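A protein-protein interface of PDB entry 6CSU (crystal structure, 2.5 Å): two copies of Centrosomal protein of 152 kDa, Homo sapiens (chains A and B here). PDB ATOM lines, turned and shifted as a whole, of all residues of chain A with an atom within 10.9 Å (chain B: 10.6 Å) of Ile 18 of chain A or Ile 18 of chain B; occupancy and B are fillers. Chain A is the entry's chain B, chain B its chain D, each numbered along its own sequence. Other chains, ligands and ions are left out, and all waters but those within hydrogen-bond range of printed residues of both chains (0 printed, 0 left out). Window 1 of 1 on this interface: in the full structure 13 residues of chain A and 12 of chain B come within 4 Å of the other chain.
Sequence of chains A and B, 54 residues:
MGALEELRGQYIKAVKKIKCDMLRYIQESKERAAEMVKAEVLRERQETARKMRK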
ATOM      1  N   GLN A  10     -10.127  -0.370 -18.905  1.00  0.00           N
ATOM      2  CA  GLN A  10      -9.825  -0.516 -17.484  1.00  0.00           C
ATOM      3  C   GLN A  10      -8.967   0.637 -16.982  1.00  0.00           C
ATOM      4  O   GLN A  10      -9.252   1.227 -15.935  1.00  0.00           O
ATOM      5  CB  GLN A  10      -9.138  -1.857 -17.224  1.00  0.00           C
ATOM      6  CG  GLN A  10     -10.075  -3.041 -17.281  1.00  0.00           C
ATOM      7  CD  GLN A  10      -9.432  -4.319 -16.789  1.00  0.00           C
ATOM      8  OE1 GLN A  10      -8.265  -4.333 -16.396  1.00  0.00           O
ATOM      9  NE2 GLN A  10     -10.195  -5.406 -16.807  1.00  0.00           N
ATOM     10  N   TYR A  11      -7.897   0.961 -17.711  1.00  0.00           N
ATOM     11  CA  TYR A  11      -7.064   2.104 -17.356  1.00  0.00           C
ATOM     12  C   TYR A  11      -7.883   3.388 -17.311  1.00  0.00           C
ATOM     13  O   TYR A  11      -7.714   4.214 -16.410  1.00  0.00           O
ATOM     14  CB  TYR A  11      -5.913   2.243 -18.352  1.00  0.00           C
ATOM     15  CG  TYR A  11      -4.816   1.218 -18.193  1.00  0.00           C
ATOM     16  CD1 TYR A  11      -4.548   0.640 -16.960  1.00  0.00           C
ATOM     17  CD2 TYR A  11      -4.043   0.830 -19.280  1.00  0.00           C
ATOM     18  CE1 TYR A  11      -3.541  -0.295 -16.816  1.00  0.00           C
ATOM     19  CE2 TYR A  11      -3.037  -0.100 -19.146  1.00  0.00           C
ATOM     20  CZ  TYR A  11      -2.792  -0.663 -17.914  1.00  0.00           C
ATOM     21  OH  TYR A  11      -1.789  -1.590 -17.774  1.00  0.00           O
ATOM     22  N   ILE A  12      -8.775   3.567 -18.285  1.00  0.00           N
ATOM     23  CA  ILE A  12      -9.643   4.740 -18.306  1.00  0.00           C
ATOM     24  C   ILE A  12     -10.536   4.761 -17.074  1.00  0.00           C
ATOM     25  O   ILE A  12     -10.638   5.776 -16.377  1.00  0.00           O
ATOM     26  CB  ILE A  12     -10.473   4.763 -19.602  1.00  0.00           C
ATOM     27  CG1 ILE A  12      -9.569   5.014 -20.811  1.00  0.00           C
ATOM     28  CG2 ILE A  12     -11.580   5.810 -19.510  1.00  0.00           C
ATOM     29  CD1 ILE A  12     -10.278   4.862 -22.142  1.00  0.00           C
ATOM     30  N   LYS A  13     -11.195   3.635 -16.782  1.00  0.00           N
ATOM     31  CA  LYS A  13     -12.075   3.578 -15.621  1.00  0.00           C
ATOM     32  C   LYS A  13     -11.298   3.745 -14.322  1.00  0.00           C
ATOM     33  O   LYS A  13     -11.842   4.257 -13.337  1.00  0.00           O
ATOM     34  CB  LYS A  13     -12.853   2.260 -15.610  1.00  0.00           C
ATOM     35  CG  LYS A  13     -12.423   1.295 -14.511  1.00  0.00           C
ATOM     36  CD  LYS A  13     -12.350  -0.139 -15.014  1.00  0.00           C
ATOM     37  CE  LYS A  13     -11.733  -1.057 -13.965  1.00  0.00           C
ATOM     38  NZ  LYS A  13     -10.291  -0.764 -13.716  1.00  0.00           N
ATOM     39  N   ALA A  14     -10.030   3.327 -14.301  1.00  0.00           N
ATOM     40  CA  ALA A  14      -9.237   3.462 -13.085  1.00  0.00           C
ATOM     41  C   ALA A  14      -8.885   4.918 -12.820  1.00  0.00           C
ATOM     42  O   ALA A  14      -8.960   5.384 -11.677  1.00  0.00           O
ATOM     43  CB  ALA A  14      -7.972   2.613 -13.178  1.00  0.00           C
ATOM     44  N   VAL A  15      -8.497   5.651 -13.864  1.00  0.00           N
ATOM     45  CA  VAL A  15      -8.149   7.055 -13.689  1.00  0.00           C
ATOM     46  C   VAL A  15      -9.388   7.874 -13.353  1.00  0.00           C
ATOM     47  O   VAL A  15      -9.321   8.836 -12.578  1.00  0.00           O
ATOM     48  CB  VAL A  15      -7.437   7.594 -14.943  1.00  0.00           C
ATOM     49  CG1 VAL A  15      -7.074   9.060 -14.752  1.00  0.00           C
ATOM     50  CG2 VAL A  15      -6.194   6.781 -15.238  1.00  0.00           C
ATOM     51  N   LYS A  16     -10.536   7.514 -13.935  1.00  0.00           N
ATOM     52  CA  LYS A  16     -11.773   8.228 -13.635  1.00  0.00           C
ATOM     53  C   LYS A  16     -12.153   8.077 -12.169  1.00  0.00           C
ATOM     54  O   LYS A  16     -12.707   9.004 -11.567  1.00  0.00           O
ATOM     55  CB  LYS A  16     -12.905   7.729 -14.531  1.00  0.00           C
ATOM     56  CG  LYS A  16     -12.936   8.334 -15.916  1.00  0.00           C
ATOM     57  CD  LYS A  16     -14.286   8.083 -16.570  1.00  0.00           C
ATOM     58  CE  LYS A  16     -14.249   8.393 -18.055  1.00  0.00           C
ATOM     59  NZ  LYS A  16     -15.405   7.786 -18.776  1.00  0.00           N
ATOM     60  N   LYS A  17     -11.880   6.904 -11.588  1.00  0.00           N
ATOM     61  CA  LYS A  17     -12.024   6.714 -10.148  1.00  0.00           C
ATOM     62  C   LYS A  17     -11.150   7.700  -9.386  1.00  0.00           C
ATOM     63  O   LYS A  17     -11.611   8.376  -8.463  1.00  0.00           O
ATOM     64  CB  LYS A  17     -11.652   5.279  -9.764  1.00  0.00           C
ATOM     65  CG  LYS A  17     -12.786   4.264  -9.787  1.00  0.00           C
ATOM     66  CD  LYS A  17     -12.327   2.976 -10.473  1.00  0.00           C
ATOM     67  CE  LYS A  17     -12.889   1.727  -9.835  1.00  0.00           C
ATOM     68  NZ  LYS A  17     -12.324   0.506 -10.484  1.00  0.00           N
ATOM     69  N   ILE A  18      -9.868   7.776  -9.764  1.00  0.00           N
ATOM     70  CA  ILE A  18      -8.961   8.758  -9.175  1.00  0.00           C
ATOM     71  C   ILE A  18      -9.574  10.148  -9.249  1.00  0.00           C
ATOM     72  O   ILE A  18      -9.521  10.922  -8.289  1.00  0.00           O
ATOM     73  CB  ILE A  18      -7.591   8.712  -9.879  1.00  0.00           C
ATOM     74  CG1 ILE A  18      -6.928   7.340  -9.719  1.00  0.00           C
ATOM     75  CG2 ILE A  18      -6.690   9.828  -9.358  1.00  0.00           C
ATOM     76  CD1 ILE A  18      -6.261   7.121  -8.380  1.00  0.00           C
ATOM     77  N   LYS A  19     -10.185  10.472 -10.391  1.00  0.00           N
ATOM     78  CA  LYS A  19     -10.826  11.771 -10.557  1.00  0.00           C
ATOM     79  C   LYS A  19     -11.986  11.946  -9.586  1.00  0.00           C
ATOM     80  O   LYS A  19     -12.174  13.030  -9.026  1.00  0.00           O
ATOM     81  CB  LYS A  19     -11.305  11.927 -11.996  1.00  0.00           C
ATOM     82  CG  LYS A  19     -11.934  13.269 -12.294  1.00  0.00           C
ATOM     83  CD  LYS A  19     -13.170  13.093 -13.148  1.00  0.00           C
ATOM     84  CE  LYS A  19     -13.503  14.369 -13.884  1.00  0.00           C
ATOM     85  NZ  LYS A  19     -14.519  14.135 -14.946  1.00  0.00           N
ATOM     86  N   CYS A  20     -12.780  10.890  -9.383  1.00  0.00           N
ATOM     87  CA  CYS A  20     -13.884  10.962  -8.429  1.00  0.00           C
ATOM     88  C   CYS A  20     -13.379  11.273  -7.029  1.00  0.00           C
ATOM     89  O   CYS A  20     -13.948  12.115  -6.325  1.00  0.00           O
ATOM     90  CB  CYS A  20     -14.669   9.651  -8.426  1.00  0.00           C
ATOM     91  SG  CYS A  20     -15.605   9.331  -9.920  1.00  0.00           S
ATOM     92  N   ASP A  21     -12.314  10.590  -6.604  1.00  0.00           N
ATOM     93  CA  ASP A  21     -11.740  10.851  -5.289  1.00  0.00           C
ATOM     94  C   ASP A  21     -11.312  12.309  -5.161  1.00  0.00           C
ATOM     95  O   ASP A  21     -11.591  12.964  -4.149  1.00  0.00           O
ATOM     96  CB  ASP A  21     -10.554   9.917  -5.036  1.00  0.00           C
ATOM     97  CG  ASP A  21     -10.958   8.451  -4.994  1.00  0.00           C
ATOM     98  OD1 ASP A  21     -12.140   8.169  -4.707  1.00  0.00           O
ATOM     99  OD2 ASP A  21     -10.092   7.581  -5.249  1.00  0.00           O
ATOM    100  N   MET A  22     -10.642  12.839  -6.189  1.00  0.00           N
ATOM    101  CA  MET A  22     -10.215  14.234  -6.151  1.00  0.00           C
ATOM    102  C   MET A  22     -11.410  15.173  -6.158  1.00  0.00           C
ATOM    103  O   MET A  22     -11.373  16.241  -5.539  1.00  0.00           O
ATOM    104  CB  MET A  22      -9.296  14.536  -7.335  1.00  0.00           C
ATOM    105  CG  MET A  22      -8.110  13.599  -7.477  1.00  0.00           C
ATOM    106  SD  MET A  22      -6.993  13.554  -6.060  1.00  0.00           S
ATOM    107  CE  MET A  22      -7.525  12.068  -5.211  1.00  0.00           C
ATOM    108  N   LEU A  23     -12.478  14.794  -6.861  1.00  0.00           N
ATOM    109  CA  LEU A  23     -13.681  15.616  -6.902  1.00  0.00           C
ATOM    110  C   LEU A  23     -14.317  15.718  -5.526  1.00  0.00           C
ATOM    111  O   LEU A  23     -14.531  16.818  -5.006  1.00  0.00           O
ATOM    112  CB  LEU A  23     -14.675  15.039  -7.907  1.00  0.00           C
ATOM    113  CG  LEU A  23     -14.870  15.873  -9.169  1.00  0.00           C
ATOM    114  CD1 LEU A  23     -13.623  15.813 -10.023  1.00  0.00           C
ATOM    115  CD2 LEU A  23     -16.081  15.390  -9.944  1.00  0.00           C
ATOM    116  N   ARG A  24     -14.637  14.565  -4.925  1.00  0.00           N
ATOM    117  CA  ARG A  24     -15.194  14.538  -3.577  1.00  0.00           C
ATOM    118  C   ARG A  24     -14.359  15.375  -2.623  1.00  0.00           C
ATOM    119  O   ARG A  24     -14.892  16.100  -1.778  1.00  0.00           O
ATOM    120  CB  ARG A  24     -15.285  13.097  -3.070  1.00  0.00           C
ATOM    121  CG  ARG A  24     -16.018  12.141  -3.987  1.00  0.00           C
ATOM    122  CD  ARG A  24     -17.277  11.603  -3.336  1.00  0.00           C
ATOM    123  NE  ARG A  24     -18.364  12.577  -3.372  1.00  0.00           N
ATOM    124  CZ  ARG A  24     -19.587  12.354  -2.901  1.00  0.00           C
ATOM    125  NH1 ARG A  24     -19.891  11.183  -2.353  1.00  0.00           N
ATOM    126  NH2 ARG A  24     -20.508  13.304  -2.984  1.00  0.00           N
ATOM    127  N   TYR A  25     -13.035  15.288  -2.753  1.00  0.00           N
ATOM    128  CA  TYR A  25     -12.151  16.109  -1.936  1.00  0.00           C
ATOM    129  C   TYR A  25     -12.407  17.592  -2.174  1.00  0.00           C
ATOM    130  O   TYR A  25     -12.591  18.365  -1.226  1.00  0.00           O
ATOM    131  CB  TYR A  25     -10.699  15.755  -2.243  1.00  0.00           C
ATOM    132  CG  TYR A  25      -9.693  16.568  -1.473  1.00  0.00           C
ATOM    133  CD1 TYR A  25      -9.345  16.220  -0.180  1.00  0.00           C
ATOM    134  CD2 TYR A  25      -9.084  17.679  -2.043  1.00  0.00           C
ATOM    135  CE1 TYR A  25      -8.423  16.952   0.530  1.00  0.00           C
ATOM    136  CE2 TYR A  25      -8.158  18.417  -1.343  1.00  0.00           C
ATOM    137  CZ  TYR A  25      -7.830  18.049  -0.055  1.00  0.00           C
ATOM    138  OH  TYR A  25      -6.908  18.782   0.652  1.00  0.00           O
ATOM    139  N   ILE A  26     -12.426  18.005  -3.443  1.00  0.00           N
ATOM    140  CA  ILE A  26     -12.568  19.420  -3.779  1.00  0.00           C
ATOM    141  C   ILE A  26     -13.923  19.950  -3.327  1.00  0.00           C
ATOM    142  O   ILE A  26     -14.031  21.085  -2.842  1.00  0.00           O
ATOM    143  CB  ILE A  26     -12.348  19.627  -5.289  1.00  0.00           C
ATOM    144  CG1 ILE A  26     -10.858  19.530  -5.619  1.00  0.00           C
ATOM    145  CG2 ILE A  26     -12.907  20.966  -5.741  1.00  0.00           C
ATOM    146  CD1 ILE A  26     -10.580  19.153  -7.060  1.00  0.00           C
ATOM    147  N   GLN B  10       1.035   4.940 -20.472  1.00  0.00           N
ATOM    148  CA  GLN B  10       0.097   6.049 -20.583  1.00  0.00           C
ATOM    149  C   GLN B  10      -0.730   6.200 -19.316  1.00  0.00           C
ATOM    150  O   GLN B  10      -1.014   7.323 -18.885  1.00  0.00           O
ATOM    151  CB  GLN B  10      -0.812   5.844 -21.793  1.00  0.00           C
ATOM    152  CG  GLN B  10      -0.095   5.854 -23.129  1.00  0.00           C
ATOM    153  CD  GLN B  10      -0.903   5.182 -24.218  1.00  0.00           C
ATOM    154  OE1 GLN B  10      -1.950   4.591 -23.952  1.00  0.00           O
ATOM    155  NE2 GLN B  10      -0.419   5.264 -25.455  1.00  0.00           N
ATOM    156  N   TYR B  11      -1.138   5.083 -18.712  1.00  0.00           N
ATOM    157  CA  TYR B  11      -1.846   5.162 -17.440  1.00  0.00           C
ATOM    158  C   TYR B  11      -0.978   5.827 -16.381  1.00  0.00           C
ATOM    159  O   TYR B  11      -1.417   6.756 -15.692  1.00  0.00           O
ATOM    160  CB  TYR B  11      -2.271   3.769 -16.977  1.00  0.00           C
ATOM    161  CG  TYR B  11      -2.796   3.762 -15.557  1.00  0.00           C
ATOM    162  CD1 TYR B  11      -1.947   3.542 -14.476  1.00  0.00           C
ATOM    163  CD2 TYR B  11      -4.139   3.986 -15.293  1.00  0.00           C
ATOM    164  CE1 TYR B  11      -2.422   3.544 -13.180  1.00  0.00           C
ATOM    165  CE2 TYR B  11      -4.624   3.984 -13.998  1.00  0.00           C
ATOM    166  CZ  TYR B  11      -3.759   3.766 -12.946  1.00  0.00           C
ATOM    167  OH  TYR B  11      -4.235   3.763 -11.655  1.00  0.00           O
ATOM    168  N   ILE B  12       0.263   5.353 -16.239  1.00  0.00           N
ATOM    169  CA  ILE B  12       1.169   5.880 -15.221  1.00  0.00           C
ATOM    170  C   ILE B  12       1.374   7.373 -15.413  1.00  0.00           C
ATOM    171  O   ILE B  12       1.372   8.149 -14.448  1.00  0.00           O
ATOM    172  CB  ILE B  12       2.508   5.118 -15.256  1.00  0.00           C
ATOM    173  CG1 ILE B  12       2.312   3.656 -14.845  1.00  0.00           C
ATOM    174  CG2 ILE B  12       3.547   5.800 -14.376  1.00  0.00           C
ATOM    175  CD1 ILE B  12       1.814   3.475 -13.430  1.00  0.00           C
ATOM    176  N   LYS B  13       1.546   7.802 -16.664  1.00  0.00           N
ATOM    177  CA  LYS B  13       1.742   9.222 -16.935  1.00  0.00           C
ATOM    178  C   LYS B  13       0.509  10.029 -16.554  1.00  0.00           C
ATOM    179  O   LYS B  13       0.628  11.120 -15.980  1.00  0.00           O
ATOM    180  CB  LYS B  13       2.087   9.438 -18.410  1.00  0.00           C
ATOM    181  CG  LYS B  13       2.103  10.904 -18.815  1.00  0.00           C
ATOM    182  CD  LYS B  13       1.818  11.103 -20.289  1.00  0.00           C
ATOM    183  CE  LYS B  13       3.004  10.710 -21.138  1.00  0.00           C
ATOM    184  NZ  LYS B  13       2.840  11.185 -22.540  1.00  0.00           N
ATOM    185  N   ALA B  14      -0.682   9.508 -16.859  1.00  0.00           N
ATOM    186  CA  ALA B  14      -1.911  10.216 -16.517  1.00  0.00           C
ATOM    187  C   ALA B  14      -2.008  10.447 -15.017  1.00  0.00           C
ATOM    188  O   ALA B  14      -2.254  11.569 -14.568  1.00  0.00           O
ATOM    189  CB  ALA B  14      -3.129   9.439 -17.020  1.00  0.00           C
ATOM    190  N   VAL B  15      -1.795   9.394 -14.224  1.00  0.00           N
ATOM    191  CA  VAL B  15      -1.966   9.512 -12.779  1.00  0.00           C
ATOM    192  C   VAL B  15      -0.843  10.336 -12.160  1.00  0.00           C
ATOM    193  O   VAL B  15      -1.064  11.053 -11.176  1.00  0.00           O
ATOM    194  CB  VAL B  15      -2.074   8.117 -12.129  1.00  0.00           C
ATOM    195  CG1 VAL B  15      -3.118   7.269 -12.842  1.00  0.00           C
ATOM    196  CG2 VAL B  15      -0.730   7.411 -12.125  1.00  0.00           C
ATOM    197  N   LYS B  16       0.370  10.265 -12.719  1.00  0.00           N
ATOM    198  CA  LYS B  16       1.466  11.061 -12.178  1.00  0.00           C
ATOM    199  C   LYS B  16       1.259  12.544 -12.447  1.00  0.00           C
ATOM    200  O   LYS B  16       1.781  13.384 -11.709  1.00  0.00           O
ATOM    201  CB  LYS B  16       2.804  10.588 -12.751  1.00  0.00           C
ATOM    202  CG  LYS B  16       3.488   9.514 -11.915  1.00  0.00           C
ATOM    203  CD  LYS B  16       4.623   8.836 -12.676  1.00  0.00           C
ATOM    204  CE  LYS B  16       5.756   9.799 -12.999  1.00  0.00           C
ATOM    205  NZ  LYS B  16       6.772   9.168 -13.892  1.00  0.00           N
ATOM    206  N   LYS B  17       0.505  12.882 -13.494  1.00  0.00           N
ATOM    207  CA  LYS B  17       0.136  14.274 -13.722  1.00  0.00           C
ATOM    208  C   LYS B  17      -0.968  14.713 -12.774  1.00  0.00           C
ATOM    209  O   LYS B  17      -0.984  15.863 -12.324  1.00  0.00           O
ATOM    210  CB  LYS B  17      -0.308  14.479 -15.169  1.00  0.00           C
ATOM    211  CG  LYS B  17       0.833  14.567 -16.155  1.00  0.00           C
ATOM    212  CD  LYS B  17       0.325  14.816 -17.563  1.00  0.00           C
ATOM    213  CE  LYS B  17       1.481  14.871 -18.546  1.00  0.00           C
ATOM    214  NZ  LYS B  17       1.024  15.061 -19.949  1.00  0.00           N
ATOM    215  N   ILE B  18      -1.907  13.814 -12.475  1.00  0.00           N
ATOM    216  CA  ILE B  18      -2.968  14.130 -11.524  1.00  0.00           C
ATOM    217  C   ILE B  18      -2.377  14.386 -10.146  1.00  0.00           C
ATOM    218  O   ILE B  18      -2.793  15.306  -9.433  1.00  0.00           O
ATOM    219  CB  ILE B  18      -4.010  12.996 -11.504  1.00  0.00           C
ATOM    220  CG1 ILE B  18      -4.800  12.976 -12.817  1.00  0.00           C
ATOM    221  CG2 ILE B  18      -4.947  13.126 -10.312  1.00  0.00           C
ATOM    222  CD1 ILE B  18      -5.852  11.899 -12.858  1.00  0.00           C
ATOM    223  N   LYS B  19      -1.378  13.592  -9.761  1.00  0.00           N
ATOM    224  CA  LYS B  19      -0.717  13.793  -8.478  1.00  0.00           C
ATOM    225  C   LYS B  19       0.045  15.112  -8.452  1.00  0.00           C
ATOM    226  O   LYS B  19       0.006  15.837  -7.452  1.00  0.00           O
ATOM    227  CB  LYS B  19       0.219  12.620  -8.195  1.00  0.00           C
ATOM    228  CG  LYS B  19       1.109  12.789  -6.983  1.00  0.00           C
ATOM    229  CD  LYS B  19       2.071  11.612  -6.871  1.00  0.00           C
ATOM    230  CE  LYS B  19       3.004  11.760  -5.683  1.00  0.00           C
ATOM    231  NZ  LYS B  19       3.933  10.602  -5.572  1.00  0.00           N
ATOM    232  N   CYS B  20       0.740  15.442  -9.544  1.00  0.00           N
ATOM    233  CA  CYS B  20       1.441  16.721  -9.604  1.00  0.00           C
ATOM    234  C   CYS B  20       0.469  17.884  -9.486  1.00  0.00           C
ATOM    235  O   CYS B  20       0.770  18.890  -8.831  1.00  0.00           O
ATOM    236  CB  CYS B  20       2.242  16.826 -10.901  1.00  0.00           C
ATOM    237  SG  CYS B  20       3.743  15.822 -10.926  1.00  0.00           S
ATOM    238  N   ASP B  21      -0.703  17.768 -10.114  1.00  0.00           N
ATOM    239  CA  ASP B  21      -1.696  18.831 -10.025  1.00  0.00           C
ATOM    240  C   ASP B  21      -2.243  18.957  -8.609  1.00  0.00           C
ATOM    241  O   ASP B  21      -2.392  20.071  -8.095  1.00  0.00           O
ATOM    242  CB  ASP B  21      -2.827  18.583 -11.024  1.00  0.00           C
ATOM    243  CG  ASP B  21      -2.450  18.968 -12.445  1.00  0.00           C
ATOM    244  OD1 ASP B  21      -1.382  19.591 -12.631  1.00  0.00           O
ATOM    245  OD2 ASP B  21      -3.228  18.664 -13.372  1.00  0.00           O
ATOM    246  N   MET B  22      -2.534  17.827  -7.957  1.00  0.00           N
ATOM    247  CA  MET B  22      -3.062  17.873  -6.597  1.00  0.00           C
ATOM    248  C   MET B  22      -2.015  18.367  -5.608  1.00  0.00           C
ATOM    249  O   MET B  22      -2.341  19.098  -4.665  1.00  0.00           O
ATOM    250  CB  MET B  22      -3.570  16.496  -6.184  1.00  0.00           C
ATOM    251  CG  MET B  22      -4.768  16.032  -6.973  1.00  0.00           C
ATOM    252  SD  MET B  22      -6.158  17.183  -6.891  1.00  0.00           S
ATOM    253  CE  MET B  22      -6.508  17.194  -5.133  1.00  0.00           C
ATOM    254  N   LEU B  23      -0.756  17.965  -5.801  1.00  0.00           N
ATOM    255  CA  LEU B  23       0.326  18.444  -4.946  1.00  0.00           C
ATOM    256  C   LEU B  23       0.412  19.965  -4.966  1.00  0.00           C
ATOM    257  O   LEU B  23       0.571  20.606  -3.921  1.00  0.00           O
ATOM    258  CB  LEU B  23       1.654  17.832  -5.393  1.00  0.00           C
ATOM    259  CG  LEU B  23       1.931  16.394  -4.959  1.00  0.00           C
ATOM    260  CD1 LEU B  23       3.233  15.869  -5.555  1.00  0.00           C
ATOM    261  CD2 LEU B  23       1.973  16.340  -3.454  1.00  0.00           C
ATOM    262  N   ARG B  24       0.316  20.559  -6.157  1.00  0.00           N
ATOM    263  CA  ARG B  24       0.394  22.012  -6.266  1.00  0.00           C
ATOM    264  C   ARG B  24      -0.886  22.673  -5.771  1.00  0.00           C
ATOM    265  O   ARG B  24      -0.837  23.730  -5.131  1.00  0.00           O
ATOM    266  CB  ARG B  24       0.679  22.414  -7.712  1.00  0.00           C
ATOM    267  CG  ARG B  24       2.149  22.653  -8.023  1.00  0.00           C
ATOM    268  CD  ARG B  24       2.698  23.877  -7.289  1.00  0.00           C
ATOM    269  NE  ARG B  24       3.588  23.519  -6.185  1.00  0.00           N
ATOM    270  CZ  ARG B  24       4.322  24.393  -5.503  1.00  0.00           C
ATOM    271  NH1 ARG B  24       4.279  25.681  -5.816  1.00  0.00           N
ATOM    272  NH2 ARG B  24       5.100  23.980  -4.511  1.00  0.00           N
ATOM    273  N   TYR B  25      -2.040  22.073  -6.069  1.00  0.00           N
ATOM    274  CA  TYR B  25      -3.306  22.602  -5.568  1.00  0.00           C
ATOM    275  C   TYR B  25      -3.325  22.627  -4.046  1.00  0.00           C
ATOM    276  O   TYR B  25      -3.801  23.592  -3.437  1.00  0.00           O
ATOM    277  CB  TYR B  25      -4.464  21.766  -6.116  1.00  0.00           C
ATOM    278  CG  TYR B  25      -5.803  21.958  -5.427  1.00  0.00           C
ATOM    279  CD1 TYR B  25      -6.659  22.990  -5.796  1.00  0.00           C
ATOM    280  CD2 TYR B  25      -6.227  21.084  -4.429  1.00  0.00           C
ATOM    281  CE1 TYR B  25      -7.891  23.158  -5.176  1.00  0.00           C
ATOM    282  CE2 TYR B  25      -7.457  21.246  -3.801  1.00  0.00           C
ATOM    283  CZ  TYR B  25      -8.287  22.284  -4.179  1.00  0.00           C
ATOM    284  OH  TYR B  25      -9.510  22.449  -3.560  1.00  0.00           O
ATOM    285  N   ILE B  26      -2.792  21.579  -3.416  1.00  0.00           N
ATOM    286  CA  ILE B  26      -2.803  21.486  -1.961  1.00  0.00           C
ATOM    287  C   ILE B  26      -1.845  22.503  -1.349  1.00  0.00           C
ATOM    288  O   ILE B  26      -2.208  23.245  -0.427  1.00  0.00           O
ATOM    289  CB  ILE B  26      -2.458  20.052  -1.521  1.00  0.00           C
ATOM    290  CG1 ILE B  26      -3.666  19.132  -1.714  1.00  0.00           C
ATOM    291  CG2 ILE B  26      -1.967  20.032  -0.081  1.00  0.00           C
ATOM    292  CD1 ILE B  26      -3.362  17.674  -1.473  1.00  0.00           C
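Hydrophobic or aromatic side chains of chain B within 4 Å of the printed part of chain A: Tyr 11, Val 15, Ile 18, Met 22 and Tyr 25. Of the 17 printed residues of chain A, 7 touch a printed residue of chain B. Hydrophobic or aromatic side chains of chain A within 4 Å of the printed part of chain B: Tyr 11, Ala 14, Val 15, Ile 18, Met 22, Tyr 25 and Ile 26. Among the printed residues, no Asp or Glu carboxylate lies within 4 Å of a Lys or Arg side-chain nitrogen of the other chain.
Ala 14 of chain A touches just one residue of chain B: Tyr 11 (3.7 Å). Val 15 of chain A touches just these residues of chain B: Tyr 11 (3.4 Å), Val 15 (3.9 Å) and Ile 18 (3.6 Å). Lys 17 of chain A touches none of the printed residues of chain B. Ile 18 of chain A touches just one residue of chain B: Ile 18. No residue of chain B comes within 4 Å of Cys 20 of chain A. No residue of chain B comes within 4 Å of Asp 21 of chain A. Of the printed residues of chain B, Ile 26 of chain A touches Tyr 25. Of the printed residues of chain A, Tyr 11 of chain B touches Tyr 11 (3.8 Å), Ala 14 (3.7 Å) and Val 15 (3.4 Å). No residue of chain A comes within 4 Å of Ala 14 of chain B. Val 15 of chain B touches just one residue of chain A: Val 15 (3.9 Å). Lys 16 of chain B touches none of the printed residues of chain A. No residue of chain A comes within 4 Å of Cys 20 of chain B. No residue of chain A comes within 4 Å of Asp 21 of chain B. Of the printed residues of chain A, Tyr 25 of chain B touches Tyr 25 (3.8 Å) and Ile 26 (3.8 Å). The nearest residue of chain B that does not touch Ile 18 of chain A is Tyr 11 of chain B (4.9 Å). The nearest printed residue of chain B that does not touch Tyr 11 of chain A is Gln 10 of chain B (6.3 Å).
Among the printed residues, merely in contact across the chains: Val 15 of chain A with Tyr 11 of chain B, Met 22 of chain A with Met 22 of chain B, Val 15 of chain A with Ile 18 of chain B, Ala 14 of chain A with Tyr 11 of chain B, Tyr 11 of chain A with Tyr 11 of chain B, Tyr 25 of chain A with Tyr 25 of chain B, Ile 26 of chain A with Tyr 25 of chain B, Ile 18 of chain A with Ile 18 of chain B and Val 15 of chain A with Val 15 of chain B.
Ala 14 of chain A touches Tyr 11 of chain B, but with the chains exchanged Tyr 11 of chain A does not touch Ala 14 of chain B (7.0 Å). Ile 18 of chain A touches its own counterpart, Ile 18 of chain B. Met 22 of chain A touches its own counterpart, Met 22 of chain B. Tyr 25 of chain B touches its own counterpart, Tyr 25 of chain A. Of the 9 pairs that touch across the chains among the printed residues, 5 have their exchanged pair printed and touching as well.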
